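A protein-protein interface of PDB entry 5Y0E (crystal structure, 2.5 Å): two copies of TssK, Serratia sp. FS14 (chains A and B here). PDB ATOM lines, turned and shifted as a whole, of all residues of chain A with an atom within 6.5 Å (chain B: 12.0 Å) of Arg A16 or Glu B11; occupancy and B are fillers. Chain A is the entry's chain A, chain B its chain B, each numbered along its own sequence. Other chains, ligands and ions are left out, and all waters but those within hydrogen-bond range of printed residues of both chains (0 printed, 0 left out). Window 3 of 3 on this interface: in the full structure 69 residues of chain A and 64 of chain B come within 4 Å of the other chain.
The side-chain amide nitrogen of Gln A21 lies within hydrogen-bond range of the backbone carbonyl oxygen of Trp B9 (3.4 Å). The side-chain carboxylate of Glu B11 lies within salt-bridge range of the guanidinium group of Arg A16 (3.2 Å).
Leu A15 touches Leu B15. CB of Pro A17 touches O of Trp B9 (3.5 Å). C of Thr B10 touches CG of Pro A17, 3.7 Å away. CG of Pro A17 touches CA of Glu B11, 3.6 Å away. Phe A20 touches Trp B9 (CB to CD2, 3.4 Å). CZ of Phe A20 touches CD2 of Leu B15, 3.9 Å away. Phe A20 touches Phe B20.
Arg A16 touches just one residue of chain B: Glu B11. Printed residues of chain A within 4 Å of Glu B11: Arg A16 (3.2 Å) and Pro A17 (3.6 Å). No residue of chain B comes within 4 Å of Phe A14. Leu A15 touches just one residue of chain B: Leu B15. Of chain B, only Trp B9, Thr B10 and Glu B11 come within 4 Å of Pro A17. No residue of chain B comes within 4 Å of His A18. No residue of chain B comes within 4 Å of His A19. Printed residues of chain A within 4 Å of Leu B15: Leu A15 (3.96 Å) and Phe A20 (3.9 Å). Printed residues of chain B within 4 Å of Gln A21: Trp B9. Of the printed residues of chain A, Phe B20 touches Phe A20.
Leu B15 touches its own counterpart, Leu A15. Phe A20 touches Leu B15, but with the chains exchanged Leu A15 does not touch Phe B20 (6.2 Å). Phe B20 touches its own counterpart, Phe A20. 5 positions are printed for both chains. Of the 9 pairs that touch across the chains among the printed residues, 2 have their exchanged pair printed and touching as well.
N of Arg A16 sits at hydrogen-bond distance from ND1 of His A19, at 3.0 Å. The backbone carbonyl oxygen of Val B7 is in hydrogen-bond range of the indole nitrogen of Trp B9 (3.4 Å).
Of the 8 printed residues of chain A, 5 touch a printed residue of chain B. Hydrophobic or aromatic side chains of chain A within 4 Å of the printed part of chain B: Leu A15, Pro A17 and Phe A20. Along chain A the printed residues that touch a printed residue of chain B span positions 15 to 21. Of the 12 printed residues of chain B, 5 touch a printed residue of chain A. Among the printed residues, 9 pairs touch across the chains.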
ATOM      1  N   PHE A  14      -0.877  -8.034 -19.948  1.00  0.00           N
ATOM      2  CA  PHE A  14       0.290  -8.558 -19.266  1.00  0.00           C
ATOM      3  C   PHE A  14       1.452  -8.640 -20.248  1.00  0.00           C
ATOM      4  O   PHE A  14       1.319  -9.218 -21.331  1.00  0.00           O
ATOM      5  CB  PHE A  14       0.014  -9.922 -18.653  1.00  0.00           C
ATOM      6  CG  PHE A  14       1.173 -10.455 -17.908  1.00  0.00           C
ATOM      7  CD1 PHE A  14       1.838  -9.655 -17.000  1.00  0.00           C
ATOM      8  CD2 PHE A  14       1.636 -11.725 -18.138  1.00  0.00           C
ATOM      9  CE1 PHE A  14       2.928 -10.119 -16.319  1.00  0.00           C
ATOM     10  CE2 PHE A  14       2.728 -12.200 -17.458  1.00  0.00           C
ATOM     11  CZ  PHE A  14       3.377 -11.392 -16.546  1.00  0.00           C
ATOM     12  N   LEU A  15       2.558  -7.990 -19.938  1.00  0.00           N
ATOM     13  CA  LEU A  15       3.670  -7.982 -20.859  1.00  0.00           C
ATOM     14  C   LEU A  15       4.505  -9.233 -20.847  1.00  0.00           C
ATOM     15  O   LEU A  15       4.847  -9.743 -19.816  1.00  0.00           O
ATOM     16  CB  LEU A  15       4.591  -6.793 -20.598  1.00  0.00           C
ATOM     17  CG  LEU A  15       4.150  -5.370 -20.885  1.00  0.00           C
ATOM     18  CD1 LEU A  15       5.188  -4.389 -20.421  1.00  0.00           C
ATOM     19  CD2 LEU A  15       3.865  -5.157 -22.343  1.00  0.00           C
ATOM     20  N   ARG A  16       4.839  -9.707 -22.032  1.00  0.00           N
ATOM     21  CA  ARG A  16       5.692 -10.858 -22.194  1.00  0.00           C
ATOM     22  C   ARG A  16       6.758 -10.548 -23.237  1.00  0.00           C
ATOM     23  O   ARG A  16       6.718  -9.527 -23.871  1.00  0.00           O
ATOM     24  CB  ARG A  16       4.877 -12.083 -22.529  1.00  0.00           C
ATOM     25  CG  ARG A  16       4.474 -12.824 -21.281  1.00  0.00           C
ATOM     26  CD  ARG A  16       3.645 -14.031 -21.581  1.00  0.00           C
ATOM     27  NE  ARG A  16       4.445 -15.224 -21.518  1.00  0.00           N
ATOM     28  CZ  ARG A  16       3.980 -16.423 -21.805  1.00  0.00           C
ATOM     29  NH1 ARG A  16       2.723 -16.573 -22.150  1.00  0.00           N
ATOM     30  NH2 ARG A  16       4.765 -17.474 -21.734  1.00  0.00           N
ATOM     31  N   PRO A  17       7.746 -11.417 -23.390  1.00  0.00           N
ATOM     32  CA  PRO A  17       8.812 -11.131 -24.342  1.00  0.00           C
ATOM     33  C   PRO A  17       8.295 -11.066 -25.753  1.00  0.00           C
ATOM     34  O   PRO A  17       8.723 -10.282 -26.544  1.00  0.00           O
ATOM     35  CB  PRO A  17       9.742 -12.323 -24.180  1.00  0.00           C
ATOM     36  CG  PRO A  17       9.377 -12.935 -22.894  1.00  0.00           C
ATOM     37  CD  PRO A  17       7.929 -12.711 -22.740  1.00  0.00           C
ATOM     38  N   HIS A  18       7.357 -11.925 -26.040  1.00  0.00           N
ATOM     39  CA  HIS A  18       6.738 -12.002 -27.331  1.00  0.00           C
ATOM     40  C   HIS A  18       6.272 -10.665 -27.907  1.00  0.00           C
ATOM     41  O   HIS A  18       6.386 -10.451 -29.087  1.00  0.00           O
ATOM     42  CB  HIS A  18       5.579 -12.967 -27.259  1.00  0.00           C
ATOM     43  CG  HIS A  18       5.866 -14.197 -26.468  1.00  0.00           C
ATOM     44  ND1 HIS A  18       7.133 -14.572 -26.099  1.00  0.00           N
ATOM     45  CD2 HIS A  18       5.039 -15.131 -25.955  1.00  0.00           C
ATOM     46  CE1 HIS A  18       7.078 -15.684 -25.402  1.00  0.00           C
ATOM     47  NE2 HIS A  18       5.819 -16.047 -25.300  1.00  0.00           N
ATOM     48  N   HIS A  19       5.708  -9.790 -27.092  1.00  0.00           N
ATOM     49  CA  HIS A  19       5.303  -8.497 -27.549  1.00  0.00           C
ATOM     50  C   HIS A  19       6.439  -7.748 -28.192  1.00  0.00           C
ATOM     51  O   HIS A  19       6.321  -7.291 -29.294  1.00  0.00           O
ATOM     52  CB  HIS A  19       4.773  -7.692 -26.390  1.00  0.00           C
ATOM     53  CG  HIS A  19       3.538  -8.260 -25.802  1.00  0.00           C
ATOM     54  ND1 HIS A  19       3.480  -8.724 -24.517  1.00  0.00           N
ATOM     55  CD2 HIS A  19       2.320  -8.468 -26.333  1.00  0.00           C
ATOM     56  CE1 HIS A  19       2.278  -9.195 -24.279  1.00  0.00           C
ATOM     57  NE2 HIS A  19       1.553  -9.051 -25.366  1.00  0.00           N
ATOM     58  N   PHE A  20       7.543  -7.605 -27.498  1.00  0.00           N
ATOM     59  CA  PHE A  20       8.644  -6.884 -28.058  1.00  0.00           C
ATOM     60  C   PHE A  20       9.206  -7.573 -29.270  1.00  0.00           C
ATOM     61  O   PHE A  20       9.619  -6.942 -30.196  1.00  0.00           O
ATOM     62  CB  PHE A  20       9.706  -6.704 -27.008  1.00  0.00           C
ATOM     63  CG  PHE A  20       9.225  -5.971 -25.820  1.00  0.00           C
ATOM     64  CD1 PHE A  20       8.522  -6.618 -24.847  1.00  0.00           C
ATOM     65  CD2 PHE A  20       9.451  -4.635 -25.689  1.00  0.00           C
ATOM     66  CE1 PHE A  20       8.063  -5.950 -23.756  1.00  0.00           C
ATOM     67  CE2 PHE A  20       8.997  -3.957 -24.598  1.00  0.00           C
ATOM     68  CZ  PHE A  20       8.298  -4.620 -23.630  1.00  0.00           C
ATOM     69  N   GLN A  21       9.214  -8.884 -29.247  1.00  0.00           N
ATOM     70  CA  GLN A  21       9.716  -9.661 -30.365  1.00  0.00           C
ATOM     71  C   GLN A  21       8.906  -9.394 -31.625  1.00  0.00           C
ATOM     72  O   GLN A  21       9.452  -9.007 -32.661  1.00  0.00           O
ATOM     73  CB  GLN A  21       9.689 -11.141 -29.998  1.00  0.00           C
ATOM     74  CG  GLN A  21      10.603 -11.503 -28.854  1.00  0.00           C
ATOM     75  CD  GLN A  21      10.500 -12.963 -28.477  1.00  0.00           C
ATOM     76  OE1 GLN A  21       9.637 -13.682 -28.966  1.00  0.00           O
ATOM     77  NE2 GLN A  21      11.362 -13.398 -27.583  1.00  0.00           N
ATOM     78  N   VAL B   7      18.194  -5.838 -29.401  1.00  0.00           N
ATOM     79  CA  VAL B   7      17.961  -6.241 -28.024  1.00  0.00           C
ATOM     80  C   VAL B   7      17.332  -7.621 -28.022  1.00  0.00           C
ATOM     81  O   VAL B   7      16.468  -7.921 -28.851  1.00  0.00           O
ATOM     82  CB  VAL B   7      17.054  -5.210 -27.331  1.00  0.00           C
ATOM     83  CG1 VAL B   7      16.589  -5.705 -25.985  1.00  0.00           C
ATOM     84  CG2 VAL B   7      17.762  -3.890 -27.216  1.00  0.00           C
ATOM     85  N   VAL B   8      17.780  -8.477 -27.114  1.00  0.00           N
ATOM     86  CA  VAL B   8      17.131  -9.756 -26.872  1.00  0.00           C
ATOM     87  C   VAL B   8      16.201  -9.584 -25.692  1.00  0.00           C
ATOM     88  O   VAL B   8      16.584  -9.003 -24.674  1.00  0.00           O
ATOM     89  CB  VAL B   8      18.150 -10.873 -26.600  1.00  0.00           C
ATOM     90  CG1 VAL B   8      17.432 -12.145 -26.211  1.00  0.00           C
ATOM     91  CG2 VAL B   8      19.000 -11.114 -27.811  1.00  0.00           C
ATOM     92  N   TRP B   9      14.985 -10.066 -25.831  1.00  0.00           N
ATOM     93  CA  TRP B   9      13.974  -9.957 -24.793  1.00  0.00           C
ATOM     94  C   TRP B   9      13.706 -11.357 -24.257  1.00  0.00           C
ATOM     95  O   TRP B   9      13.150 -12.201 -24.961  1.00  0.00           O
ATOM     96  CB  TRP B   9      12.702  -9.319 -25.346  1.00  0.00           C
ATOM     97  CG  TRP B   9      12.945  -8.104 -26.186  1.00  0.00           C
ATOM     98  CD1 TRP B   9      13.228  -8.078 -27.508  1.00  0.00           C
ATOM     99  CD2 TRP B   9      12.898  -6.740 -25.763  1.00  0.00           C
ATOM    100  NE1 TRP B   9      13.371  -6.795 -27.938  1.00  0.00           N
ATOM    101  CE2 TRP B   9      13.173  -5.951 -26.884  1.00  0.00           C
ATOM    102  CE3 TRP B   9      12.641  -6.110 -24.546  1.00  0.00           C
ATOM    103  CZ2 TRP B   9      13.211  -4.566 -26.828  1.00  0.00           C
ATOM    104  CZ3 TRP B   9      12.677  -4.742 -24.494  1.00  0.00           C
ATOM    105  CH2 TRP B   9      12.958  -3.982 -25.622  1.00  0.00           C
ATOM    106  N   THR B  10      14.095 -11.612 -23.026  1.00  0.00           N
ATOM    107  CA  THR B  10      13.908 -12.924 -22.451  1.00  0.00           C
ATOM    108  C   THR B  10      12.799 -12.978 -21.446  1.00  0.00           C
ATOM    109  O   THR B  10      12.389 -11.980 -20.925  1.00  0.00           O
ATOM    110  CB  THR B  10      15.165 -13.373 -21.742  1.00  0.00           C
ATOM    111  OG1 THR B  10      15.621 -12.322 -20.905  1.00  0.00           O
ATOM    112  CG2 THR B  10      16.214 -13.668 -22.732  1.00  0.00           C
ATOM    113  N   GLU B  11      12.304 -14.168 -21.185  1.00  0.00           N
ATOM    114  CA  GLU B  11      11.263 -14.320 -20.220  1.00  0.00           C
ATOM    115  C   GLU B  11      11.857 -14.125 -18.864  1.00  0.00           C
ATOM    116  O   GLU B  11      12.913 -14.623 -18.567  1.00  0.00           O
ATOM    117  CB  GLU B  11      10.629 -15.680 -20.313  1.00  0.00           C
ATOM    118  CG  GLU B  11       9.387 -15.785 -19.471  1.00  0.00           C
ATOM    119  CD  GLU B  11       8.127 -15.628 -20.270  1.00  0.00           C
ATOM    120  OE1 GLU B  11       8.108 -16.038 -21.428  1.00  0.00           O
ATOM    121  OE2 GLU B  11       7.150 -15.104 -19.742  1.00  0.00           O
ATOM    122  N   GLY B  12      11.164 -13.346 -18.057  1.00  0.00           N
ATOM    123  CA  GLY B  12      11.575 -13.046 -16.714  1.00  0.00           C
ATOM    124  C   GLY B  12      12.450 -11.841 -16.662  1.00  0.00           C
ATOM    125  O   GLY B  12      12.952 -11.509 -15.625  1.00  0.00           O
ATOM    126  N   MET B  13      12.615 -11.161 -17.779  1.00  0.00           N
ATOM    127  CA  MET B  13      13.484 -10.004 -17.828  1.00  0.00           C
ATOM    128  C   MET B  13      12.883  -8.796 -17.168  1.00  0.00           C
ATOM    129  O   MET B  13      11.708  -8.548 -17.273  1.00  0.00           O
ATOM    130  CB  MET B  13      13.848  -9.667 -19.260  1.00  0.00           C
ATOM    131  CG  MET B  13      14.980  -8.684 -19.413  1.00  0.00           C
ATOM    132  SD  MET B  13      15.235  -8.202 -21.106  1.00  0.00           S
ATOM    133  CE  MET B  13      16.606  -9.252 -21.469  1.00  0.00           C
ATOM    134  N   PHE B  14      13.725  -8.051 -16.485  1.00  0.00           N
ATOM    135  CA  PHE B  14      13.303  -6.866 -15.813  1.00  0.00           C
ATOM    136  C   PHE B  14      13.513  -5.717 -16.744  1.00  0.00           C
ATOM    137  O   PHE B  14      14.619  -5.374 -17.019  1.00  0.00           O
ATOM    138  CB  PHE B  14      14.156  -6.668 -14.592  1.00  0.00           C
ATOM    139  CG  PHE B  14      13.829  -5.442 -13.834  1.00  0.00           C
ATOM    140  CD1 PHE B  14      12.605  -5.285 -13.266  1.00  0.00           C
ATOM    141  CD2 PHE B  14      14.743  -4.447 -13.707  1.00  0.00           C
ATOM    142  CE1 PHE B  14      12.295  -4.158 -12.572  1.00  0.00           C
ATOM    143  CE2 PHE B  14      14.441  -3.310 -13.016  1.00  0.00           C
ATOM    144  CZ  PHE B  14      13.215  -3.170 -12.442  1.00  0.00           C
ATOM    145  N   LEU B  15      12.442  -5.108 -17.211  1.00  0.00           N
ATOM    146  CA  LEU B  15      12.547  -4.008 -18.136  1.00  0.00           C
ATOM    147  C   LEU B  15      13.106  -2.795 -17.503  1.00  0.00           C
ATOM    148  O   LEU B  15      12.735  -2.431 -16.432  1.00  0.00           O
ATOM    149  CB  LEU B  15      11.193  -3.654 -18.690  1.00  0.00           C
ATOM    150  CG  LEU B  15      10.472  -4.759 -19.408  1.00  0.00           C
ATOM    151  CD1 LEU B  15       9.009  -4.432 -19.371  1.00  0.00           C
ATOM    152  CD2 LEU B  15      10.954  -4.797 -20.829  1.00  0.00           C
ATOM    153  N   ARG B  16      14.048  -2.180 -18.181  1.00  0.00           N
ATOM    154  CA  ARG B  16      14.713  -0.970 -17.743  1.00  0.00           C
ATOM    155  C   ARG B  16      14.677   0.005 -18.885  1.00  0.00           C
ATOM    156  O   ARG B  16      14.420  -0.376 -20.037  1.00  0.00           O
ATOM    157  CB  ARG B  16      16.144  -1.287 -17.298  1.00  0.00           C
ATOM    158  CG  ARG B  16      16.164  -2.295 -16.173  1.00  0.00           C
ATOM    159  CD  ARG B  16      17.417  -2.219 -15.351  1.00  0.00           C
ATOM    160  NE  ARG B  16      17.720  -0.852 -14.981  1.00  0.00           N
ATOM    161  CZ  ARG B  16      18.871  -0.485 -14.447  1.00  0.00           C
ATOM    162  NH1 ARG B  16      19.801  -1.396 -14.227  1.00  0.00           N
ATOM    163  NH2 ARG B  16      19.093   0.783 -14.139  1.00  0.00           N
ATOM    164  N   HIS B  19      16.547  -0.786 -22.254  1.00  0.00           N
ATOM    165  CA  HIS B  19      16.041  -1.710 -23.256  1.00  0.00           C
ATOM    166  C   HIS B  19      15.417  -0.959 -24.416  1.00  0.00           C
ATOM    167  O   HIS B  19      15.811  -1.125 -25.574  1.00  0.00           O
ATOM    168  CB  HIS B  19      15.035  -2.657 -22.617  1.00  0.00           C
ATOM    169  CG  HIS B  19      15.659  -3.689 -21.733  1.00  0.00           C
ATOM    170  ND1 HIS B  19      15.831  -3.506 -20.378  1.00  0.00           N
ATOM    171  CD2 HIS B  19      16.153  -4.917 -22.014  1.00  0.00           C
ATOM    172  CE1 HIS B  19      16.400  -4.582 -19.864  1.00  0.00           C
ATOM    173  NE2 HIS B  19      16.609  -5.450 -20.836  1.00  0.00           N
ATOM    174  N   PHE B  20      14.461  -0.096 -24.115  1.00  0.00           N
ATOM    175  CA  PHE B  20      13.834   0.702 -25.150  1.00  0.00           C
ATOM    176  C   PHE B  20      14.830   1.642 -25.805  1.00  0.00           C
ATOM    177  O   PHE B  20      14.810   1.812 -27.026  1.00  0.00           O
ATOM    178  CB  PHE B  20      12.665   1.472 -24.550  1.00  0.00           C
ATOM    179  CG  PHE B  20      11.746   0.612 -23.758  1.00  0.00           C
ATOM    180  CD1 PHE B  20      10.707  -0.049 -24.367  1.00  0.00           C
ATOM    181  CD2 PHE B  20      11.946   0.431 -22.407  1.00  0.00           C
ATOM    182  CE1 PHE B  20       9.877  -0.861 -23.643  1.00  0.00           C
ATOM    183  CE2 PHE B  20      11.119  -0.376 -21.686  1.00  0.00           C
ATOM    184  CZ  PHE B  20      10.084  -1.025 -22.301  1.00  0.00           C
